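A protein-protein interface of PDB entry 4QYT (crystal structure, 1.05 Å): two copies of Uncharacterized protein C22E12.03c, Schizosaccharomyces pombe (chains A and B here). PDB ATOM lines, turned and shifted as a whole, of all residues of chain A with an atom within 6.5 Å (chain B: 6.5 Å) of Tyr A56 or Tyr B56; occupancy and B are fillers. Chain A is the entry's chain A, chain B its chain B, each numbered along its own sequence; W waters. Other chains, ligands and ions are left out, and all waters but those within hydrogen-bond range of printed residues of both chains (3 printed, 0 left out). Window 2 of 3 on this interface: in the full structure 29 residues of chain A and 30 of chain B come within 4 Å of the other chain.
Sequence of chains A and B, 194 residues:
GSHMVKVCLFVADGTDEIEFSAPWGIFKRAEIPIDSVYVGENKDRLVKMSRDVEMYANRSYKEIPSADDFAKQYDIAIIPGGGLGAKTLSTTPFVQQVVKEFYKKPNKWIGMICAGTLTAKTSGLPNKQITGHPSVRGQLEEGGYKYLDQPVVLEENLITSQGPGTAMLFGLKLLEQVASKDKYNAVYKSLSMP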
ATOM      1  N   PHE A  20      27.465  16.194  29.496  1.00  0.00           N
ATOM      2  CA  PHE A  20      26.521  15.150  29.899  1.00  0.00           C
ATOM      3  C   PHE A  20      27.267  13.941  30.488  1.00  0.00           C
ATOM      4  O   PHE A  20      26.944  13.464  31.565  1.00  0.00           O
ATOM      5  CB  PHE A  20      25.654  14.725  28.698  1.00  0.00           C
ATOM      6  CG  PHE A  20      24.640  13.643  29.031  1.00  0.00           C
ATOM      7  CD1 PHE A  20      25.044  12.303  29.165  1.00  0.00           C
ATOM      8  CD2 PHE A  20      23.318  13.964  29.304  1.00  0.00           C
ATOM      9  CE1 PHE A  20      24.136  11.310  29.516  1.00  0.00           C
ATOM     10  CE2 PHE A  20      22.419  12.994  29.664  1.00  0.00           C
ATOM     11  CZ  PHE A  20      22.841  11.678  29.794  1.00  0.00           C
ATOM     12  N   SER A  36      18.428  10.417  33.015  1.00  0.00           N
ATOM     13  CA  SER A  36      18.436  11.532  32.080  1.00  0.00           C
ATOM     14  C   SER A  36      17.002  11.892  31.767  1.00  0.00           C
ATOM     15  O   SER A  36      16.159  11.023  31.522  1.00  0.00           O
ATOM     16  CB  SER A  36      19.218  11.192  30.815  1.00  0.00           C
ATOM     17  OG  SER A  36      18.702  10.017  30.208  1.00  0.00           O
ATOM     18  N   ASN A  42      10.989  15.548  20.616  1.00  0.00           N
ATOM     19  CA  ASN A  42      11.031  14.192  20.125  1.00  0.00           C
ATOM     20  C   ASN A  42      10.202  13.245  21.013  1.00  0.00           C
ATOM     21  O   ASN A  42      10.590  12.901  22.121  1.00  0.00           O
ATOM     22  CB  ASN A  42      12.490  13.712  19.993  1.00  0.00           C
ATOM     23  CG  ASN A  42      12.577  12.364  19.315  1.00  0.00           C
ATOM     24  OD1 ASN A  42      12.281  11.330  19.922  1.00  0.00           O
ATOM     25  ND2 ASN A  42      12.815  12.382  18.014  1.00  0.00           N
ATOM     26  N   ASP A  44      10.076  10.035  21.089  1.00  0.00           N
ATOM     27  CA  ASP A  44      10.712   8.751  21.368  1.00  0.00           C
ATOM     28  C   ASP A  44      11.876   8.894  22.352  1.00  0.00           C
ATOM     29  O   ASP A  44      12.587   7.932  22.605  1.00  0.00           O
ATOM     30  CB  ASP A  44      11.203   8.107  20.060  1.00  0.00           C
ATOM     31  CG  ASP A  44      10.080   7.842  19.089  1.00  0.00           C
ATOM     32  OD1 ASP A  44       8.981   7.466  19.560  1.00  0.00           O
ATOM     33  OD2 ASP A  44      10.222   8.244  17.917  1.00  0.00           O
ATOM     34  N   ARG A  45      12.072  10.128  22.810  1.00  0.00           N
ATOM     35  CA  ARG A  45      13.158  10.502  23.712  1.00  0.00           C
ATOM     36  C   ARG A  45      14.508  10.319  23.062  1.00  0.00           C
ATOM     37  O   ARG A  45      15.485   9.982  23.730  1.00  0.00           O
ATOM     38  CB  ARG A  45      13.108   9.703  25.003  1.00  0.00           C
ATOM     39  CG  ARG A  45      11.745   9.740  25.669  1.00  0.00           C
ATOM     40  CD  ARG A  45      11.806   9.051  27.012  1.00  0.00           C
ATOM     41  NE  ARG A  45      12.461   7.750  26.912  1.00  0.00           N
ATOM     42  CZ  ARG A  45      11.831   6.637  26.581  1.00  0.00           C
ATOM     43  NH1 ARG A  45      10.562   6.693  26.239  1.00  0.00           N
ATOM     44  NH2 ARG A  45      12.498   5.500  26.466  1.00  0.00           N
ATOM     45  N   LEU A  46      14.528  10.458  21.743  1.00  0.00           N
ATOM     46  CA  LEU A  46      15.773  10.416  21.012  1.00  0.00           C
ATOM     47  C   LEU A  46      16.294  11.832  20.909  1.00  0.00           C
ATOM     48  O   LEU A  46      15.640  12.720  20.365  1.00  0.00           O
ATOM     49  CB  LEU A  46      15.578   9.783  19.633  1.00  0.00           C
ATOM     50  CG  LEU A  46      16.862   9.727  18.791  1.00  0.00           C
ATOM     51  CD1 LEU A  46      17.945   8.880  19.455  1.00  0.00           C
ATOM     52  CD2 LEU A  46      16.557   9.207  17.392  1.00  0.00           C
ATOM     53  N   VAL A  47      17.492  12.037  21.436  1.00  0.00           N
ATOM     54  CA  VAL A  47      18.092  13.354  21.539  1.00  0.00           C
ATOM     55  C   VAL A  47      19.227  13.482  20.525  1.00  0.00           C
ATOM     56  O   VAL A  47      20.061  12.586  20.406  1.00  0.00           O
ATOM     57  CB  VAL A  47      18.686  13.530  22.940  1.00  0.00           C
ATOM     58  CG1 VAL A  47      19.132  14.968  23.110  1.00  0.00           C
ATOM     59  CG2 VAL A  47      17.685  13.136  24.016  1.00  0.00           C
ATOM     60  N   ASP A  52      26.244  16.013  17.555  1.00  0.00           N
ATOM     61  CA  ASP A  52      25.598  15.071  16.666  1.00  0.00           C
ATOM     62  C   ASP A  52      25.520  13.629  17.146  1.00  0.00           C
ATOM     63  O   ASP A  52      25.023  12.790  16.415  1.00  0.00           O
ATOM     64  CB  ASP A  52      26.181  15.120  15.244  1.00  0.00           C
ATOM     65  CG  ASP A  52      26.200  16.504  14.698  1.00  0.00           C
ATOM     66  OD1 ASP A  52      25.143  17.154  14.758  1.00  0.00           O
ATOM     67  OD2 ASP A  52      27.276  16.964  14.270  1.00  0.00           O
ATOM     68  N   VAL A  53      25.876  13.333  18.379  1.00  0.00           N
ATOM     69  CA  VAL A  53      25.519  12.022  18.920  1.00  0.00           C
ATOM     70  C   VAL A  53      23.997  11.929  19.045  1.00  0.00           C
ATOM     71  O   VAL A  53      23.364  12.874  19.468  1.00  0.00           O
ATOM     72  CB  VAL A  53      26.173  11.803  20.294  1.00  0.00           C
ATOM     73  CG1 VAL A  53      25.535  10.663  21.068  1.00  0.00           C
ATOM     74  CG2 VAL A  53      27.646  11.538  20.115  1.00  0.00           C
ATOM     75  N   GLU A  54      23.442  10.775  18.667  1.00  0.00           N
ATOM     76  CA  GLU A  54      22.034  10.487  18.899  1.00  0.00           C
ATOM     77  C   GLU A  54      21.892   9.455  19.998  1.00  0.00           C
ATOM     78  O   GLU A  54      22.390   8.331  19.889  1.00  0.00           O
ATOM     79  CB  GLU A  54      21.385  10.021  17.605  1.00  0.00           C
ATOM     80  CG  GLU A  54      21.466  11.091  16.535  1.00  0.00           C
ATOM     81  CD  GLU A  54      20.808  10.765  15.243  1.00  0.00           C
ATOM     82  OE1 GLU A  54      19.929   9.916  15.234  1.00  0.00           O
ATOM     83  OE2 GLU A  54      20.999  11.569  14.321  1.00  0.00           O
ATOM     84  N   MET A  55      21.299   9.920  21.116  1.00  0.00           N
ATOM     85  CA  MET A  55      21.198   9.199  22.422  1.00  0.00           C
ATOM     86  C   MET A  55      19.725   9.125  22.885  1.00  0.00           C
ATOM     87  O   MET A  55      19.128  10.204  22.923  1.00  0.00           O
ATOM     88  CB  MET A  55      22.012   9.945  23.511  1.00  0.00           C
ATOM     89  CG  MET A  55      21.936   9.375  24.919  1.00  0.00           C
ATOM     90  SD  MET A  55      22.959  10.329  26.078  1.00  0.00           S
ATOM     91  CE  MET A  55      21.812  11.644  26.274  1.00  0.00           C
ATOM     92  N   TYR A  56      19.258   8.000  23.483  1.00  0.00           N
ATOM     93  CA  TYR A  56      17.945   7.940  24.179  1.00  0.00           C
ATOM     94  C   TYR A  56      18.045   8.412  25.599  1.00  0.00           C
ATOM     95  O   TYR A  56      18.827   7.928  26.398  1.00  0.00           O
ATOM     96  CB  TYR A  56      17.374   6.523  24.242  1.00  0.00           C
ATOM     97  CG  TYR A  56      16.855   6.048  22.925  1.00  0.00           C
ATOM     98  CD1 TYR A  56      15.624   6.472  22.440  1.00  0.00           C
ATOM     99  CD2 TYR A  56      17.600   5.169  22.159  1.00  0.00           C
ATOM    100  CE1 TYR A  56      15.191   6.051  21.201  1.00  0.00           C
ATOM    101  CE2 TYR A  56      17.118   4.671  20.972  1.00  0.00           C
ATOM    102  CZ  TYR A  56      15.919   5.119  20.490  1.00  0.00           C
ATOM    103  OH  TYR A  56      15.492   4.749  19.242  1.00  0.00           O
ATOM    104  N   ALA A  57      17.204   9.370  25.924  1.00  0.00           N
ATOM    105  CA  ALA A  57      17.078   9.744  27.316  1.00  0.00           C
ATOM    106  C   ALA A  57      16.221   8.713  28.022  1.00  0.00           C
ATOM    107  O   ALA A  57      15.342   8.090  27.431  1.00  0.00           O
ATOM    108  CB  ALA A  57      16.479  11.111  27.446  1.00  0.00           C
ATOM    109  N   ASN A  58      16.396   8.600  29.336  1.00  0.00           N
ATOM    110  CA  ASN A  58      15.563   7.677  30.108  1.00  0.00           C
ATOM    111  C   ASN A  58      14.108   8.091  30.215  1.00  0.00           C
ATOM    112  O   ASN A  58      13.223   7.243  30.272  1.00  0.00           O
ATOM    113  CB  ASN A  58      16.097   7.567  31.550  1.00  0.00           C
ATOM    114  CG  ASN A  58      17.478   6.996  31.674  1.00  0.00           C
ATOM    115  OD1 ASN A  58      18.309   7.556  32.344  1.00  0.00           O
ATOM    116  ND2 ASN A  58      17.749   5.905  30.988  1.00  0.00           N
ATOM    117  N   ARG A  59      13.891   9.395  30.349  1.00  0.00           N
ATOM    118  CA  ARG A  59      12.584   9.989  30.612  1.00  0.00           C
ATOM    119  C   ARG A  59      12.407  11.238  29.775  1.00  0.00           C
ATOM    120  O   ARG A  59      13.386  11.886  29.407  1.00  0.00           O
ATOM    121  CB  ARG A  59      12.406  10.351  32.089  1.00  0.00           C
ATOM    122  CG  ARG A  59      12.685   9.218  33.052  1.00  0.00           C
ATOM    123  CD  ARG A  59      12.289   9.592  34.472  1.00  0.00           C
ATOM    124  NE  ARG A  59      10.846   9.742  34.586  1.00  0.00           N
ATOM    125  CZ  ARG A  59      10.199  10.050  35.688  1.00  0.00           C
ATOM    126  NH1 ARG A  59      10.843  10.515  36.725  1.00  0.00           N
ATOM    127  NH2 ARG A  59       8.886   9.908  35.720  1.00  0.00           N
ATOM    128  N   PHE B  20      34.513   7.916  25.185  1.00  0.00           N
ATOM    129  CA  PHE B  20      33.966   8.186  23.867  1.00  0.00           C
ATOM    130  C   PHE B  20      33.799   9.685  23.634  1.00  0.00           C
ATOM    131  O   PHE B  20      34.207  10.233  22.605  1.00  0.00           O
ATOM    132  CB  PHE B  20      32.652   7.420  23.704  1.00  0.00           C
ATOM    133  CG  PHE B  20      31.999   7.617  22.364  1.00  0.00           C
ATOM    134  CD1 PHE B  20      31.248   8.731  22.094  1.00  0.00           C
ATOM    135  CD2 PHE B  20      32.144   6.664  21.342  1.00  0.00           C
ATOM    136  CE1 PHE B  20      30.685   8.945  20.821  1.00  0.00           C
ATOM    137  CE2 PHE B  20      31.585   6.853  20.107  1.00  0.00           C
ATOM    138  CZ  PHE B  20      30.873   7.989  19.845  1.00  0.00           C
ATOM    139  N   SER B  36      31.639   7.163  14.355  1.00  0.00           N
ATOM    140  CA  SER B  36      31.659   6.071  15.296  1.00  0.00           C
ATOM    141  C   SER B  36      31.400   4.764  14.540  1.00  0.00           C
ATOM    142  O   SER B  36      30.486   4.703  13.697  1.00  0.00           O
ATOM    143  CB  SER B  36      30.657   6.301  16.403  1.00  0.00           C
ATOM    144  OG  SER B  36      29.349   6.507  15.880  1.00  0.00           O
ATOM    145  N   ASN B  42      24.108  -5.657  17.391  1.00  0.00           N
ATOM    146  CA  ASN B  42      22.803  -5.023  17.164  1.00  0.00           C
ATOM    147  C   ASN B  42      22.679  -4.475  15.719  1.00  0.00           C
ATOM    148  O   ASN B  42      23.495  -3.681  15.275  1.00  0.00           O
ATOM    149  CB  ASN B  42      22.529  -3.926  18.193  1.00  0.00           C
ATOM    150  CG  ASN B  42      21.202  -3.279  17.983  1.00  0.00           C
ATOM    151  OD1 ASN B  42      21.082  -2.331  17.192  1.00  0.00           O
ATOM    152  ND2 ASN B  42      20.170  -3.888  18.536  1.00  0.00           N
ATOM    153  N   ASP B  44      20.659  -2.434  14.345  1.00  0.00           N
ATOM    154  CA  ASP B  44      20.320  -1.040  14.227  1.00  0.00           C
ATOM    155  C   ASP B  44      21.466  -0.113  14.656  1.00  0.00           C
ATOM    156  O   ASP B  44      21.278   1.103  14.662  1.00  0.00           O
ATOM    157  CB  ASP B  44      19.077  -0.728  15.060  1.00  0.00           C
ATOM    158  CG  ASP B  44      17.889  -1.506  14.582  1.00  0.00           C
ATOM    159  OD1 ASP B  44      17.618  -1.436  13.367  1.00  0.00           O
ATOM    160  OD2 ASP B  44      17.194  -2.149  15.412  1.00  0.00           O
ATOM    161  N   ARG B  45      22.624  -0.685  14.992  1.00  0.00           N
ATOM    162  CA  ARG B  45      23.766   0.107  15.456  1.00  0.00           C
ATOM    163  C   ARG B  45      23.459   0.848  16.751  1.00  0.00           C
ATOM    164  O   ARG B  45      24.069   1.870  17.050  1.00  0.00           O
ATOM    165  CB  ARG B  45      24.291   1.072  14.386  1.00  0.00           C
ATOM    166  CG  ARG B  45      24.703   0.369  13.117  1.00  0.00           C
ATOM    167  CD  ARG B  45      25.201   1.307  12.065  1.00  0.00           C
ATOM    168  NE  ARG B  45      24.498   2.539  11.900  1.00  0.00           N
ATOM    169  CZ  ARG B  45      23.351   2.647  11.263  1.00  0.00           C
ATOM    170  NH1 ARG B  45      22.863   1.646  10.546  1.00  0.00           N
ATOM    171  NH2 ARG B  45      22.668   3.773  11.377  1.00  0.00           N
ATOM    172  N   LEU B  46      22.556   0.284  17.551  1.00  0.00           N
ATOM    173  CA  LEU B  46      22.282   0.839  18.880  1.00  0.00           C
ATOM    174  C   LEU B  46      23.194   0.162  19.868  1.00  0.00           C
ATOM    175  O   LEU B  46      23.263  -1.054  19.929  1.00  0.00           O
ATOM    176  CB  LEU B  46      20.786   0.632  19.203  1.00  0.00           C
ATOM    177  CG  LEU B  46      20.292   1.301  20.473  1.00  0.00           C
ATOM    178  CD1 LEU B  46      20.571   2.793  20.470  1.00  0.00           C
ATOM    179  CD2 LEU B  46      18.823   1.020  20.680  1.00  0.00           C
ATOM    180  N   VAL B  47      23.913   1.010  20.618  1.00  0.00           N
ATOM    181  CA  VAL B  47      24.959   0.593  21.544  1.00  0.00           C
ATOM    182  C   VAL B  47      24.498   0.823  22.960  1.00  0.00           C
ATOM    183  O   VAL B  47      23.985   1.904  23.249  1.00  0.00           O
ATOM    184  CB  VAL B  47      26.251   1.379  21.263  1.00  0.00           C
ATOM    185  CG1 VAL B  47      27.390   0.782  22.086  1.00  0.00           C
ATOM    186  CG2 VAL B  47      26.594   1.392  19.790  1.00  0.00           C
ATOM    187  N   ASP B  52      25.383   2.545  30.787  1.00  0.00           N
ATOM    188  CA  ASP B  52      23.968   2.373  30.394  1.00  0.00           C
ATOM    189  C   ASP B  52      23.393   3.443  29.486  1.00  0.00           C
ATOM    190  O   ASP B  52      22.230   3.360  29.151  1.00  0.00           O
ATOM    191  CB  ASP B  52      23.032   2.139  31.599  1.00  0.00           C
ATOM    192  CG  ASP B  52      23.520   1.023  32.435  1.00  0.00           C
ATOM    193  OD1 ASP B  52      23.774  -0.067  31.894  1.00  0.00           O
ATOM    194  OD2 ASP B  52      23.620   1.212  33.661  1.00  0.00           O
ATOM    195  N   VAL B  53      24.200   4.370  28.974  1.00  0.00           N
ATOM    196  CA  VAL B  53      23.703   5.209  27.901  1.00  0.00           C
ATOM    197  C   VAL B  53      23.412   4.333  26.686  1.00  0.00           C
ATOM    198  O   VAL B  53      24.203   3.464  26.329  1.00  0.00           O
ATOM    199  CB  VAL B  53      24.713   6.329  27.534  1.00  0.00           C
ATOM    200  CG1 VAL B  53      24.422   6.942  26.150  1.00  0.00           C
ATOM    201  CG2 VAL B  53      24.695   7.406  28.610  1.00  0.00           C
ATOM    202  N   GLU B  54      22.298   4.621  26.026  1.00  0.00           N
ATOM    203  CA  GLU B  54      21.946   3.981  24.755  1.00  0.00           C
ATOM    204  C   GLU B  54      22.102   4.972  23.645  1.00  0.00           C
ATOM    205  O   GLU B  54      21.411   5.998  23.631  1.00  0.00           O
ATOM    206  CB  GLU B  54      20.532   3.396  24.817  1.00  0.00           C
ATOM    207  CG  GLU B  54      20.510   2.172  25.707  1.00  0.00           C
ATOM    208  CD  GLU B  54      19.238   1.354  25.712  1.00  0.00           C
ATOM    209  OE1 GLU B  54      18.422   1.464  24.784  1.00  0.00           O
ATOM    210  OE2 GLU B  54      19.223   0.379  26.508  1.00  0.00           O
ATOM    211  N   MET B  55      22.961   4.714  22.665  1.00  0.00           N
ATOM    212  CA  MET B  55      23.150   5.705  21.594  1.00  0.00           C
ATOM    213  C   MET B  55      23.519   4.994  20.295  1.00  0.00           C
ATOM    214  O   MET B  55      24.070   3.891  20.373  1.00  0.00           O
ATOM    215  CB  MET B  55      24.266   6.677  21.997  1.00  0.00           C
ATOM    216  CG  MET B  55      25.605   5.992  22.212  1.00  0.00           C
ATOM    217  SD  MET B  55      26.904   7.238  22.263  1.00  0.00           S
ATOM    218  CE  MET B  55      28.056   6.204  21.371  1.00  0.00           C
ATOM    219  N   TYR B  56      23.166   5.600  19.151  1.00  0.00           N
ATOM    220  CA  TYR B  56      23.429   5.044  17.811  1.00  0.00           C
ATOM    221  C   TYR B  56      24.848   5.345  17.381  1.00  0.00           C
ATOM    222  O   TYR B  56      25.361   6.452  17.526  1.00  0.00           O
ATOM    223  CB  TYR B  56      22.501   5.634  16.749  1.00  0.00           C
ATOM    224  CG  TYR B  56      21.084   5.119  16.849  1.00  0.00           C
ATOM    225  CD1 TYR B  56      20.755   3.866  16.381  1.00  0.00           C
ATOM    226  CD2 TYR B  56      20.112   5.844  17.526  1.00  0.00           C
ATOM    227  CE1 TYR B  56      19.478   3.383  16.504  1.00  0.00           C
ATOM    228  CE2 TYR B  56      18.817   5.383  17.630  1.00  0.00           C
ATOM    229  CZ  TYR B  56      18.523   4.137  17.153  1.00  0.00           C
ATOM    230  OH  TYR B  56      17.259   3.667  17.386  1.00  0.00           O
ATOM    231  N   ALA B  57      25.497   4.328  16.847  1.00  0.00           N
ATOM    232  CA  ALA B  57      26.758   4.504  16.135  1.00  0.00           C
ATOM    233  C   ALA B  57      26.467   4.835  14.672  1.00  0.00           C
ATOM    234  O   ALA B  57      25.430   4.483  14.136  1.00  0.00           O
ATOM    235  CB  ALA B  57      27.620   3.236  16.227  1.00  0.00           C
ATOM    236  N   ASN B  58      27.423   5.494  14.029  1.00  0.00           N
ATOM    237  CA  ASN B  58      27.232   5.858  12.631  1.00  0.00           C
ATOM    238  C   ASN B  58      27.330   4.663  11.677  1.00  0.00           C
ATOM    239  O   ASN B  58      26.617   4.657  10.654  1.00  0.00           O
ATOM    240  CB  ASN B  58      28.303   6.863  12.202  1.00  0.00           C
ATOM    241  CG  ASN B  58      28.274   8.169  12.959  1.00  0.00           C
ATOM    242  OD1 ASN B  58      29.305   8.658  13.394  1.00  0.00           O
ATOM    243  ND2 ASN B  58      27.095   8.747  13.159  1.00  0.00           N
HETATM  244  O   HOH W   1      26.611  11.468  14.389  1.00  0.00           O
HETATM  245  O   HOH W   2      20.148   4.237  31.107  1.00  0.00           O
HETATM  246  O   HOH W   3      25.215   8.922  17.437  1.00  0.00           O
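N of Tyr A56 sits at hydrogen-bond distance from O of Glu B54, 2.9 Å away.
OH of Tyr A56 is in hydrogen-bond range of OH of Tyr B56, 2.8 Å away.
N of Tyr B56 lies within hydrogen-bond range of O of Glu A54, at 2.9 Å.
N of Leu B46 sits at hydrogen-bond distance from OD1 of Asn B42 (3.0 Å).
N of Val B47 sits at hydrogen-bond distance from O of Met B55, at 2.9 Å.
N of Val A47 is in hydrogen-bond range of O of Met A55, 2.9 Å away.
Met B55 touches Val A53 (SD to CG1, 3.9 Å).
O of Glu A54 touches CA of Met B55 (3.2 Å).
Met A55 touches Val B53 (CG to CG1, 3.7 Å).
O of Glu B54 touches CA of Met A55, 3.4 Å away.
Met A55 touches Met B55.
Leu B46 touches Tyr A56.
Of the printed residues of chain B, Tyr A56 touches Leu B46, Glu B54 and Tyr B56.
Of the printed residues of chain A, Tyr B56 touches Glu A54 (2.9 Å) and Tyr A56 (2.8 Å).
Of the printed residues of chain A, Leu B46 touches Tyr A56.
Of the printed residues of chain A, Met B55 touches Val A53, Glu A54 and Met A55.
Of the printed residues of chain B, Met A55 touches Val B53 (3.7 Å), Glu B54 (3.4 Å) and Met B55 (3.99 Å).
Of the printed residues of chain B, Val A53 touches Met B55 (3.9 Å).
Printed residues of chain A within 4 Å of Val B53: Met A55.
Asn B58 touches none of the printed residues of chain A.
Ala B57 touches none of the printed residues of chain A.
The nearest printed residue of chain A that does not touch Val B53 is Phe A20 (4.05 Å).
Of the 14 printed residues of chain B, 5 touch a printed residue of chain A.
Printed residues of chain B that touch a printed residue of chain A: Leu B46, Val B53, Glu B54, Met B55 and Tyr B56.
Hydrophobic or aromatic side chains of chain B that line the printed part of chain A: Leu B46, Val B53, Met B55 and Tyr B56.
Among the printed residues, 9 pairs touch across the chains.
Among the printed residues, no Asp or Glu carboxylate lies within 4 Å of a Lys or Arg side-chain nitrogen of the other chain.
Val A53 touches Met B55, and with the chains exchanged Met A55 touches Val B53.
Glu A54 touches Met B55, and with the chains exchanged Met A55 touches Glu B54.
Glu A54 touches Tyr B56, and with the chains exchanged Tyr A56 touches Glu B54.
Tyr B56 touches its own counterpart, Tyr A56.
Positions printed for both chains: 20, 36, 42, 44, 45, 46, 47, 52, 53, 54, 55, 56, 57 and 58.
Water W3 bridges O of Tyr B56 (2.5 Å) and N of Glu A54 (2.8 Å).
Water W1 bridges the backbone carbonyl oxygen of Asp A52 (2.9 Å) and the side-chain amide nitrogen of Asn B58 (3.0 Å).
Water W2 bridges ND2 of Asn A58 (2.9 Å) and O of Asp B52 (3.0 Å).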
